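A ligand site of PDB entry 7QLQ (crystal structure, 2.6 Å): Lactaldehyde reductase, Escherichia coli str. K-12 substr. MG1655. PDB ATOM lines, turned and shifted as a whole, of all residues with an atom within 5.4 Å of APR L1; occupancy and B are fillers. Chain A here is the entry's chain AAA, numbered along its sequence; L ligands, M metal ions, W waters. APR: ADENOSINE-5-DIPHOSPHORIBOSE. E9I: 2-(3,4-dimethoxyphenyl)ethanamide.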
ATOM      1  N   ASP A  39      -6.080  29.244 -35.873  1.00  0.00           N
ATOM      2  CA  ASP A  39      -6.304  30.711 -35.763  1.00  0.00           C
ATOM      3  C   ASP A  39      -4.958  31.390 -35.509  1.00  0.00           C
ATOM      4  O   ASP A  39      -3.989  30.672 -35.192  1.00  0.00           O
ATOM      5  CB  ASP A  39      -7.363  31.048 -34.707  1.00  0.00           C
ATOM      6  CG  ASP A  39      -7.035  30.534 -33.311  1.00  0.00           C
ATOM      7  OD1 ASP A  39      -5.890  30.745 -32.879  1.00  0.00           O
ATOM      8  OD2 ASP A  39      -7.945  29.930 -32.681  1.00  0.00           O
ATOM      9  N   THR A  41      -3.749  33.353 -33.118  1.00  0.00           N
ATOM     10  CA  THR A  41      -3.247  33.252 -31.719  1.00  0.00           C
ATOM     11  C   THR A  41      -2.339  32.029 -31.579  1.00  0.00           C
ATOM     12  O   THR A  41      -1.269  32.168 -30.967  1.00  0.00           O
ATOM     13  CB  THR A  41      -4.387  33.132 -30.706  1.00  0.00           C
ATOM     14  OG1 THR A  41      -5.360  34.137 -30.986  1.00  0.00           O
ATOM     15  CG2 THR A  41      -3.931  33.268 -29.274  1.00  0.00           C
ATOM     16  N   LEU A  42      -2.782  30.880 -32.095  1.00  0.00           N
ATOM     17  CA  LEU A  42      -2.138  29.561 -31.869  1.00  0.00           C
ATOM     18  C   LEU A  42      -0.830  29.477 -32.672  1.00  0.00           C
ATOM     19  O   LEU A  42       0.089  28.778 -32.208  1.00  0.00           O
ATOM     20  CB  LEU A  42      -3.101  28.439 -32.255  1.00  0.00           C
ATOM     21  CG  LEU A  42      -4.334  28.290 -31.353  1.00  0.00           C
ATOM     22  CD1 LEU A  42      -5.342  27.337 -31.979  1.00  0.00           C
ATOM     23  CD2 LEU A  42      -3.947  27.812 -29.959  1.00  0.00           C
ATOM     24  N   CYS A  45       1.743  31.744 -30.748  1.00  0.00           N
ATOM     25  CA  CYS A  45       1.972  31.175 -29.397  1.00  0.00           C
ATOM     26  C   CYS A  45       2.874  29.937 -29.519  1.00  0.00           C
ATOM     27  O   CYS A  45       3.261  29.387 -28.469  1.00  0.00           O
ATOM     28  CB  CYS A  45       0.663  30.839 -28.691  1.00  0.00           C
ATOM     29  SG  CYS A  45      -0.090  32.284 -27.897  1.00  0.00           S
ATOM     30  N   VAL A  47       2.089  27.021 -30.724  1.00  0.00           N
ATOM     31  CA  VAL A  47       1.291  25.781 -30.469  1.00  0.00           C
ATOM     32  C   VAL A  47       1.243  24.989 -31.785  1.00  0.00           C
ATOM     33  O   VAL A  47       1.511  23.774 -31.760  1.00  0.00           O
ATOM     34  CB  VAL A  47      -0.119  26.110 -29.940  1.00  0.00           C
ATOM     35  CG1 VAL A  47      -0.968  24.867 -29.797  1.00  0.00           C
ATOM     36  CG2 VAL A  47      -0.072  26.866 -28.617  1.00  0.00           C
ATOM     37  N   PRO A  70     -13.168  33.419 -33.268  1.00  0.00           N
ATOM     38  CA  PRO A  70     -14.204  32.917 -32.365  1.00  0.00           C
ATOM     39  C   PRO A  70     -15.607  33.023 -32.996  1.00  0.00           C
ATOM     40  O   PRO A  70     -15.906  34.040 -33.579  1.00  0.00           O
ATOM     41  CB  PRO A  70     -14.095  33.834 -31.146  1.00  0.00           C
ATOM     42  CG  PRO A  70     -12.654  34.288 -31.157  1.00  0.00           C
ATOM     43  CD  PRO A  70     -12.299  34.411 -32.622  1.00  0.00           C
ATOM     44  N   ASN A  71     -16.411  31.956 -32.879  1.00  0.00           N
ATOM     45  CA  ASN A  71     -17.766  31.847 -33.485  1.00  0.00           C
ATOM     46  C   ASN A  71     -17.596  31.943 -35.003  1.00  0.00           C
ATOM     47  O   ASN A  71     -18.086  32.884 -35.631  1.00  0.00           O
ATOM     48  CB  ASN A  71     -18.730  32.881 -32.898  1.00  0.00           C
ATOM     49  CG  ASN A  71     -18.678  32.942 -31.377  1.00  0.00           C
ATOM     50  OD1 ASN A  71     -18.433  34.015 -30.816  1.00  0.00           O
ATOM     51  ND2 ASN A  71     -18.902  31.813 -30.714  1.00  0.00           N
ATOM     52  N   PRO A  72     -16.923  30.961 -35.648  1.00  0.00           N
ATOM     53  CA  PRO A  72     -16.588  31.044 -37.067  1.00  0.00           C
ATOM     54  C   PRO A  72     -17.812  31.292 -37.977  1.00  0.00           C
ATOM     55  O   PRO A  72     -18.825  30.643 -37.790  1.00  0.00           O
ATOM     56  CB  PRO A  72     -15.977  29.668 -37.390  1.00  0.00           C
ATOM     57  CG  PRO A  72     -16.483  28.765 -36.285  1.00  0.00           C
ATOM     58  CD  PRO A  72     -16.539  29.664 -35.070  1.00  0.00           C
ATOM     59  N   GLY A  96      -6.848  23.629 -32.651  1.00  0.00           N
ATOM     60  CA  GLY A  96      -7.487  24.703 -31.877  1.00  0.00           C
ATOM     61  C   GLY A  96      -8.716  24.215 -31.165  1.00  0.00           C
ATOM     62  O   GLY A  96      -8.933  22.997 -31.106  1.00  0.00           O
ATOM     63  N   GLY A  97      -9.518  25.147 -30.638  1.00  0.00           N
ATOM     64  CA  GLY A  97     -10.767  24.850 -29.916  1.00  0.00           C
ATOM     65  C   GLY A  97     -11.876  24.487 -30.870  1.00  0.00           C
ATOM     66  O   GLY A  97     -11.592  23.981 -31.966  1.00  0.00           O
ATOM     67  N   GLY A  98     -13.115  24.733 -30.454  1.00  0.00           N
ATOM     68  CA  GLY A  98     -14.321  24.489 -31.267  1.00  0.00           C
ATOM     69  C   GLY A  98     -14.296  25.242 -32.578  1.00  0.00           C
ATOM     70  O   GLY A  98     -14.773  24.674 -33.569  1.00  0.00           O
ATOM     71  N   SER A  99     -13.754  26.466 -32.586  1.00  0.00           N
ATOM     72  CA  SER A  99     -13.855  27.406 -33.748  1.00  0.00           C
ATOM     73  C   SER A  99     -13.081  26.849 -34.941  1.00  0.00           C
ATOM     74  O   SER A  99     -13.664  26.688 -36.009  1.00  0.00           O
ATOM     75  CB  SER A  99     -13.428  28.804 -33.372  1.00  0.00           C
ATOM     76  OG  SER A  99     -14.304  29.354 -32.404  1.00  0.00           O
ATOM     77  N   PRO A 100     -11.768  26.549 -34.840  1.00  0.00           N
ATOM     78  CA  PRO A 100     -11.039  25.975 -35.972  1.00  0.00           C
ATOM     79  C   PRO A 100     -11.560  24.598 -36.374  1.00  0.00           C
ATOM     80  O   PRO A 100     -11.670  24.316 -37.539  1.00  0.00           O
ATOM     81  CB  PRO A 100      -9.590  25.898 -35.465  1.00  0.00           C
ATOM     82  CG  PRO A 100      -9.538  26.955 -34.401  1.00  0.00           C
ATOM     83  CD  PRO A 100     -10.875  26.802 -33.705  1.00  0.00           C
ATOM     84  N   ASP A 102     -14.586  23.164 -35.961  1.00  0.00           N
ATOM     85  CA  ASP A 102     -15.905  23.302 -36.625  1.00  0.00           C
ATOM     86  C   ASP A 102     -15.682  23.847 -38.059  1.00  0.00           C
ATOM     87  O   ASP A 102     -16.291  23.290 -39.006  1.00  0.00           O
ATOM     88  CB  ASP A 102     -16.865  24.157 -35.788  1.00  0.00           C
ATOM     89  CG  ASP A 102     -17.399  23.451 -34.543  1.00  0.00           C
ATOM     90  OD1 ASP A 102     -17.004  22.280 -34.297  1.00  0.00           O
ATOM     91  OD2 ASP A 102     -18.233  24.064 -33.836  1.00  0.00           O
ATOM     92  N   THR A 140      -6.944  22.201 -28.616  1.00  0.00           N
ATOM     93  CA  THR A 140      -6.126  23.101 -27.776  1.00  0.00           C
ATOM     94  C   THR A 140      -6.998  23.737 -26.669  1.00  0.00           C
ATOM     95  O   THR A 140      -6.471  24.606 -25.955  1.00  0.00           O
ATOM     96  CB  THR A 140      -5.438  24.153 -28.654  1.00  0.00           C
ATOM     97  OG1 THR A 140      -6.395  25.144 -29.002  1.00  0.00           O
ATOM     98  CG2 THR A 140      -4.808  23.559 -29.898  1.00  0.00           C
ATOM     99  N   THR A 141      -8.270  23.325 -26.527  1.00  0.00           N
ATOM    100  CA  THR A 141      -9.174  23.721 -25.404  1.00  0.00           C
ATOM    101  C   THR A 141      -9.729  22.466 -24.723  1.00  0.00           C
ATOM    102  O   THR A 141      -9.691  21.398 -25.356  1.00  0.00           O
ATOM    103  CB  THR A 141     -10.308  24.649 -25.840  1.00  0.00           C
ATOM    104  OG1 THR A 141     -11.152  23.996 -26.800  1.00  0.00           O
ATOM    105  CG2 THR A 141      -9.794  25.941 -26.437  1.00  0.00           C
ATOM    106  N   THR A 144     -14.632  21.439 -26.240  1.00  0.00           N
ATOM    107  CA  THR A 144     -15.912  21.385 -26.994  1.00  0.00           C
ATOM    108  C   THR A 144     -16.118  19.957 -27.489  1.00  0.00           C
ATOM    109  O   THR A 144     -17.236  19.680 -27.919  1.00  0.00           O
ATOM    110  CB  THR A 144     -15.788  22.378 -28.156  1.00  0.00           C
ATOM    111  OG1 THR A 144     -14.656  22.002 -28.940  1.00  0.00           O
ATOM    112  CG2 THR A 144     -15.639  23.801 -27.692  1.00  0.00           C
ATOM    113  N   VAL A 153     -20.813  24.101 -35.388  1.00  0.00           N
ATOM    114  CA  VAL A 153     -21.660  25.325 -35.262  1.00  0.00           C
ATOM    115  C   VAL A 153     -20.987  26.471 -36.024  1.00  0.00           C
ATOM    116  O   VAL A 153     -19.875  26.891 -35.635  1.00  0.00           O
ATOM    117  CB  VAL A 153     -21.920  25.652 -33.782  1.00  0.00           C
ATOM    118  CG1 VAL A 153     -22.813  26.880 -33.608  1.00  0.00           C
ATOM    119  CG2 VAL A 153     -22.525  24.464 -33.082  1.00  0.00           C
ATOM    120  N   LYS A 162     -26.461  31.507 -34.944  1.00  0.00           N
ATOM    121  CA  LYS A 162     -25.585  30.310 -35.084  1.00  0.00           C
ATOM    122  C   LYS A 162     -26.467  29.114 -35.435  1.00  0.00           C
ATOM    123  O   LYS A 162     -27.529  28.982 -34.823  1.00  0.00           O
ATOM    124  CB  LYS A 162     -24.827  30.005 -33.775  1.00  0.00           C
ATOM    125  CG  LYS A 162     -23.972  31.145 -33.244  1.00  0.00           C
ATOM    126  CD  LYS A 162     -22.566  30.719 -32.837  1.00  0.00           C
ATOM    127  CE  LYS A 162     -22.509  30.006 -31.509  1.00  0.00           C
ATOM    128  NZ  LYS A 162     -21.214  29.292 -31.345  1.00  0.00           N
ATOM    129  N   MET A 181      -0.787  20.513 -25.614  1.00  0.00           N
ATOM    130  CA  MET A 181      -1.361  21.443 -26.617  1.00  0.00           C
ATOM    131  C   MET A 181      -2.289  22.444 -25.933  1.00  0.00           C
ATOM    132  O   MET A 181      -2.524  23.508 -26.531  1.00  0.00           O
ATOM    133  CB  MET A 181      -2.124  20.642 -27.684  1.00  0.00           C
ATOM    134  CG  MET A 181      -1.813  21.040 -29.112  1.00  0.00           C
ATOM    135  SD  MET A 181      -0.081  20.880 -29.585  1.00  0.00           S
ATOM    136  CE  MET A 181       0.373  19.397 -28.692  1.00  0.00           C
ATOM    137  N   MET A 182      -2.755  22.153 -24.709  1.00  0.00           N
ATOM    138  CA  MET A 182      -3.834  22.903 -23.992  1.00  0.00           C
ATOM    139  C   MET A 182      -3.274  23.813 -22.888  1.00  0.00           C
ATOM    140  O   MET A 182      -4.055  24.667 -22.399  1.00  0.00           O
ATOM    141  CB  MET A 182      -4.841  21.934 -23.360  1.00  0.00           C
ATOM    142  CG  MET A 182      -5.674  21.160 -24.372  1.00  0.00           C
ATOM    143  SD  MET A 182      -6.432  19.681 -23.663  1.00  0.00           S
ATOM    144  CE  MET A 182      -7.229  18.961 -25.097  1.00  0.00           C
ATOM    145  N   ASP A 183      -2.005  23.655 -22.496  1.00  0.00           N
ATOM    146  CA  ASP A 183      -1.435  24.283 -21.278  1.00  0.00           C
ATOM    147  C   ASP A 183      -1.416  25.810 -21.392  1.00  0.00           C
ATOM    148  O   ASP A 183      -1.477  26.467 -20.332  1.00  0.00           O
ATOM    149  CB  ASP A 183      -0.016  23.786 -20.981  1.00  0.00           C
ATOM    150  CG  ASP A 183       0.031  22.415 -20.342  1.00  0.00           C
ATOM    151  OD1 ASP A 183      -0.973  22.032 -19.679  1.00  0.00           O
ATOM    152  OD2 ASP A 183       1.052  21.735 -20.526  1.00  0.00           O
ATOM    153  N   GLY A 184      -1.340  26.349 -22.617  1.00  0.00           N
ATOM    154  CA  GLY A 184      -1.222  27.791 -22.887  1.00  0.00           C
ATOM    155  C   GLY A 184      -2.542  28.521 -22.731  1.00  0.00           C
ATOM    156  O   GLY A 184      -2.536  29.756 -22.851  1.00  0.00           O
ATOM    157  N   MET A 185      -3.645  27.811 -22.517  1.00  0.00           N
ATOM    158  CA  MET A 185      -4.972  28.409 -22.220  1.00  0.00           C
ATOM    159  C   MET A 185      -4.830  29.363 -21.036  1.00  0.00           C
ATOM    160  O   MET A 185      -4.356  28.961 -19.976  1.00  0.00           O
ATOM    161  CB  MET A 185      -6.007  27.344 -21.837  1.00  0.00           C
ATOM    162  CG  MET A 185      -6.442  26.457 -22.970  1.00  0.00           C
ATOM    163  SD  MET A 185      -7.657  25.226 -22.376  1.00  0.00           S
ATOM    164  CE  MET A 185      -9.130  26.220 -22.549  1.00  0.00           C
ATOM    165  N   PRO A 186      -5.204  30.647 -21.187  1.00  0.00           N
ATOM    166  CA  PRO A 186      -5.414  31.525 -20.034  1.00  0.00           C
ATOM    167  C   PRO A 186      -6.492  30.982 -19.085  1.00  0.00           C
ATOM    168  O   PRO A 186      -7.473  30.394 -19.534  1.00  0.00           O
ATOM    169  CB  PRO A 186      -5.830  32.851 -20.668  1.00  0.00           C
ATOM    170  CG  PRO A 186      -5.222  32.811 -22.049  1.00  0.00           C
ATOM    171  CD  PRO A 186      -5.366  31.364 -22.468  1.00  0.00           C
ATOM    172  N   LEU A 189     -10.089  31.063 -20.051  1.00  0.00           N
ATOM    173  CA  LEU A 189     -10.396  30.138 -21.174  1.00  0.00           C
ATOM    174  C   LEU A 189     -10.495  28.709 -20.632  1.00  0.00           C
ATOM    175  O   LEU A 189     -11.417  27.987 -21.038  1.00  0.00           O
ATOM    176  CB  LEU A 189      -9.320  30.278 -22.262  1.00  0.00           C
ATOM    177  CG  LEU A 189      -9.608  29.575 -23.591  1.00  0.00           C
ATOM    178  CD1 LEU A 189     -10.914  30.047 -24.225  1.00  0.00           C
ATOM    179  CD2 LEU A 189      -8.458  29.779 -24.566  1.00  0.00           C
ATOM    180  N   THR A 193     -14.182  26.954 -21.256  1.00  0.00           N
ATOM    181  CA  THR A 193     -14.201  25.677 -22.011  1.00  0.00           C
ATOM    182  C   THR A 193     -14.430  24.529 -21.031  1.00  0.00           C
ATOM    183  O   THR A 193     -15.071  23.530 -21.425  1.00  0.00           O
ATOM    184  CB  THR A 193     -12.928  25.529 -22.855  1.00  0.00           C
ATOM    185  OG1 THR A 193     -11.819  25.433 -21.963  1.00  0.00           O
ATOM    186  CG2 THR A 193     -12.721  26.676 -23.826  1.00  0.00           C
ATOM    187  N   ASP A 196     -18.103  24.505 -20.383  1.00  0.00           N
ATOM    188  CA  ASP A 196     -18.736  24.056 -21.641  1.00  0.00           C
ATOM    189  C   ASP A 196     -18.725  22.525 -21.657  1.00  0.00           C
ATOM    190  O   ASP A 196     -19.758  21.937 -21.996  1.00  0.00           O
ATOM    191  CB  ASP A 196     -18.066  24.671 -22.868  1.00  0.00           C
ATOM    192  CG  ASP A 196     -18.662  24.232 -24.197  1.00  0.00           C
ATOM    193  OD1 ASP A 196     -19.917  24.140 -24.307  1.00  0.00           O
ATOM    194  OD2 ASP A 196     -17.860  23.988 -25.114  1.00  0.00           O
ATOM    195  N   HIS A 267     -26.433  29.826 -27.920  1.00  0.00           N
ATOM    196  CA  HIS A 267     -26.106  30.079 -29.355  1.00  0.00           C
ATOM    197  C   HIS A 267     -26.528  31.475 -29.778  1.00  0.00           C
ATOM    198  O   HIS A 267     -25.731  32.192 -30.378  1.00  0.00           O
ATOM    199  CB  HIS A 267     -26.674  28.968 -30.235  1.00  0.00           C
ATOM    200  CG  HIS A 267     -25.891  27.697 -30.144  1.00  0.00           C
ATOM    201  ND1 HIS A 267     -26.417  26.483 -30.541  1.00  0.00           N
ATOM    202  CD2 HIS A 267     -24.658  27.451 -29.659  1.00  0.00           C
ATOM    203  CE1 HIS A 267     -25.519  25.540 -30.324  1.00  0.00           C
ATOM    204  NE2 HIS A 267     -24.431  26.114 -29.778  1.00  0.00           N
ATOM    205  N   HIS A 277     -18.689  30.953 -25.977  1.00  0.00           N
ATOM    206  CA  HIS A 277     -19.683  29.854 -25.861  1.00  0.00           C
ATOM    207  C   HIS A 277     -19.767  29.310 -24.433  1.00  0.00           C
ATOM    208  O   HIS A 277     -20.885  29.065 -23.938  1.00  0.00           O
ATOM    209  CB  HIS A 277     -19.336  28.794 -26.910  1.00  0.00           C
ATOM    210  CG  HIS A 277     -20.131  27.554 -26.796  1.00  0.00           C
ATOM    211  ND1 HIS A 277     -21.453  27.513 -27.129  1.00  0.00           N
ATOM    212  CD2 HIS A 277     -19.796  26.301 -26.409  1.00  0.00           C
ATOM    213  CE1 HIS A 277     -21.905  26.292 -26.945  1.00  0.00           C
ATOM    214  NE2 HIS A 277     -20.909  25.519 -26.498  1.00  0.00           N
ATOM    215  N   GLY A 278     -18.617  29.102 -23.785  1.00  0.00           N
ATOM    216  CA  GLY A 278     -18.531  28.479 -22.450  1.00  0.00           C
ATOM    217  C   GLY A 278     -19.056  29.391 -21.364  1.00  0.00           C
ATOM    218  O   GLY A 278     -19.643  28.865 -20.391  1.00  0.00           O
HETATM  219  N1  APR L   1      -3.822  28.961 -25.658  1.00  0.00           N
HETATM  220  C2  APR L   1      -4.243  30.222 -25.837  1.00  0.00           C
HETATM  221  N3  APR L   1      -5.312  30.666 -26.499  1.00  0.00           N
HETATM  222  C4  APR L   1      -6.002  29.638 -27.021  1.00  0.00           C
HETATM  223  C5  APR L   1      -5.694  28.305 -26.926  1.00  0.00           C
HETATM  224  C6  APR L   1      -4.534  27.951 -26.204  1.00  0.00           C
HETATM  225  N6  APR L   1      -4.132  26.701 -26.027  1.00  0.00           N
HETATM  226  N7  APR L   1      -6.643  27.544 -27.600  1.00  0.00           N
HETATM  227  C8  APR L   1      -7.495  28.422 -28.079  1.00  0.00           C
HETATM  228  N9  APR L   1      -7.149  29.714 -27.761  1.00  0.00           N
HETATM  229  C1' APR L   1      -7.859  30.936 -28.116  1.00  0.00           C
HETATM  230  C2' APR L   1      -8.265  31.086 -29.570  1.00  0.00           C
HETATM  231  O2' APR L   1      -7.184  31.502 -30.377  1.00  0.00           O
HETATM  232  C3' APR L   1      -9.346  32.155 -29.449  1.00  0.00           C
HETATM  233  O3' APR L   1      -8.771  33.466 -29.409  1.00  0.00           O
HETATM  234  O4' APR L   1      -9.059  30.989 -27.385  1.00  0.00           O
HETATM  235  C4' APR L   1     -10.029  31.787 -28.119  1.00  0.00           C
HETATM  236  C5' APR L   1     -11.312  31.014 -28.246  1.00  0.00           C
HETATM  237  O5' APR L   1     -11.076  29.883 -29.116  1.00  0.00           O
HETATM  238  PA  APR L   1     -12.301  28.993 -29.637  1.00  0.00           P
HETATM  239  O1A APR L   1     -11.787  28.028 -30.645  1.00  0.00           O
HETATM  240  O2A APR L   1     -13.440  29.899 -29.979  1.00  0.00           O
HETATM  241  O3A APR L   1     -12.656  28.213 -28.283  1.00  0.00           O
HETATM  242  PB  APR L   1     -13.644  27.013 -27.888  1.00  0.00           P
HETATM  243  O1B APR L   1     -12.857  25.747 -27.848  1.00  0.00           O
HETATM  244  O2B APR L   1     -14.412  27.424 -26.672  1.00  0.00           O
HETATM  245  O5D APR L   1     -14.615  26.993 -29.174  1.00  0.00           O
HETATM  246  C5D APR L   1     -15.889  27.672 -29.140  1.00  0.00           C
HETATM  247  O4D APR L   1     -16.835  25.989 -30.563  1.00  0.00           O
HETATM  248  O1D APR L   1     -18.513  24.570 -29.853  1.00  0.00           O
HETATM  249  C1D APR L   1     -18.242  25.686 -30.614  1.00  0.00           C
HETATM  250  O2D APR L   1     -20.254  27.145 -30.524  1.00  0.00           O
HETATM  251  C2D APR L   1     -18.929  26.937 -30.072  1.00  0.00           C
HETATM  252  O3D APR L   1     -18.255  28.428 -31.910  1.00  0.00           O
HETATM  253  C3D APR L   1     -18.013  28.054 -30.558  1.00  0.00           C
HETATM  254  C4D APR L   1     -16.625  27.416 -30.422  1.00  0.00           C
HETATM  255  N1  E9I L   2     -20.112  21.176 -28.887  1.00  0.00           N
HETATM  256  C7  E9I L   2     -25.171  20.313 -30.414  1.00  0.00           C
HETATM  257  C8  E9I L   2     -21.196  21.805 -29.315  1.00  0.00           C
HETATM  258  C9  E9I L   2     -24.228  16.661 -32.662  1.00  0.00           C
HETATM  259  O1  E9I L   2     -23.753  17.121 -31.401  1.00  0.00           O
HETATM  260  C1  E9I L   2     -22.814  20.656 -30.842  1.00  0.00           C
HETATM  261  C5  E9I L   2     -24.058  21.141 -30.464  1.00  0.00           C
HETATM  262  C6  E9I L   2     -25.051  18.978 -30.760  1.00  0.00           C
HETATM  263  C4  E9I L   2     -23.796  18.472 -31.166  1.00  0.00           C
HETATM  264  C3  E9I L   2     -22.702  19.313 -31.208  1.00  0.00           C
HETATM  265  O3  E9I L   2     -21.855  22.572 -28.605  1.00  0.00           O
HETATM  266  C2  E9I L   2     -21.587  21.536 -30.785  1.00  0.00           C
HETATM  267  O2  E9I L   2     -26.077  18.080 -30.737  1.00  0.00           O
HETATM  268  C10 E9I L   2     -27.303  18.457 -31.374  1.00  0.00           C
HETATM  269 FE    FE M   1     -20.839  23.385 -26.246  1.00  0.00          FE
HETATM  270  O   HOH W   1     -15.916  25.892 -24.917  1.00  0.00           O
HETATM  271  O   HOH W   2     -17.745  26.620 -33.800  1.00  0.00           O
HETATM  272  O   HOH W   3     -19.090  23.429 -27.368  1.00  0.00           O
HETATM  273  O   HOH W   4     -21.720  25.029 -29.872  1.00  0.00           O
HETATM  274  O   HOH W   5      -8.937  27.823 -31.184  1.00  0.00           O
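An oxygen (O2D) of APR L1 sits at hydrogen-bond distance from the side-chain amino group of Lys 162 (2.5 Å). The backbone NH of Ser 99 lies within hydrogen-bond range of an oxygen (O1A) of APR L1, 3.2 Å away. The side-chain hydroxyl of Ser 99 sits at hydrogen-bond distance from an oxygen (O2A) of APR L1 (2.6 Å). OG1 of Thr 141 sits at hydrogen-bond distance from O1B of APR L1 (2.7 Å). A nitrogen (N6) of APR L1 is in hydrogen-bond range of the backbone carbonyl oxygen (O) of Thr 140 (3.1 Å). OG1 of Thr 140 sits at hydrogen-bond distance from N7 of APR L1. O1B of APR L1 sits at hydrogen-bond distance from N of Gly 98 (2.8 Å). The side-chain carboxylate (OD2) of Asp 39 lies within hydrogen-bond range of an oxygen (O2') of APR L1, 2.9 Å away. OG1 of Thr 41 lies close to O2' of APR L1, at 3.3 Å. A nitrogen (N1) of APR L1 sits at hydrogen-bond distance from the backbone NH (N) of Met 185 (3.3 Å). The backbone carbonyl oxygen (O) of Thr 144 lies within hydrogen-bond range of a nitrogen (N1) of E9I L2 (3.4 Å).
The side-chain amino group of Lys 162 lies close to the side-chain amide nitrogen of Asn 71 (3.5 Å). The backbone NH (N) of Asn 71 is in hydrogen-bond range of the side-chain hydroxyl (OG) of Ser 99 (3.4 Å). The backbone NH (N) of Thr 140 sits at hydrogen-bond distance from the backbone carbonyl oxygen (O) of Gly 96, at 3.3 Å. OG1 of Thr 144 sits close to N of Gly 98, at 3.5 Å. The backbone carbonyl oxygen (O) of Leu 189 sits at hydrogen-bond distance from the side-chain hydroxyl (OG1) of Thr 193 (2.7 Å). The side-chain sulfur (SG) of Cys 45 sits close to the backbone carbonyl oxygen (O) of Thr 41. The backbone carbonyl oxygen (O) of Leu 42 lies within hydrogen-bond range of the backbone NH (N) of Val 47, at 3.0 Å. The backbone NH (N) of Val 153 is in hydrogen-bond range of the side-chain carboxylate (OD2) of Asp 102 (3.0 Å).
O of Gly 184 lies close to N1 of APR L1. Residues that only touch APR L1: Leu 42 (3.5 Å), Pro 70 (3.9 Å), Asn 71 (3.6 Å), Pro 72 (3.8 Å), Gly 97 (3.1 Å), Pro 100 (3.4 Å), Asp 102 (3.6 Å), Thr 144 (3.4 Å), Val 153 (3.95 Å), Met 181 (3.6 Å), Pro 186 (3.7 Å), Leu 189 (3.1 Å), Thr 193 (3.4 Å) and His 277 (3.5 Å). Of the 31 residues printed, 23 come within 4 Å of APR L1.
Water W4 lies within hydrogen-bond range of O2D of APR L1 (2.7 Å), O3 of E9I L2 (2.8 Å) and NE2 of His 267 (2.9 Å). Water W2 lies within hydrogen-bond range of OD2 of Asp 102, O3D of APR L1 and O of Val 153. Water W1 bridges OD2 of Asp 196 and O2B of APR L1. Water W3 lies within hydrogen-bond range of OD2 of Asp 196, O1D of APR L1 and N1 of E9I L2. Water W5 lies within hydrogen-bond range of the side-chain carboxylate of Asp 39 (2.8 Å), the backbone NH of Gly 97 (2.8 Å) and an oxygen (O1A) of APR L1 (2.9 Å).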
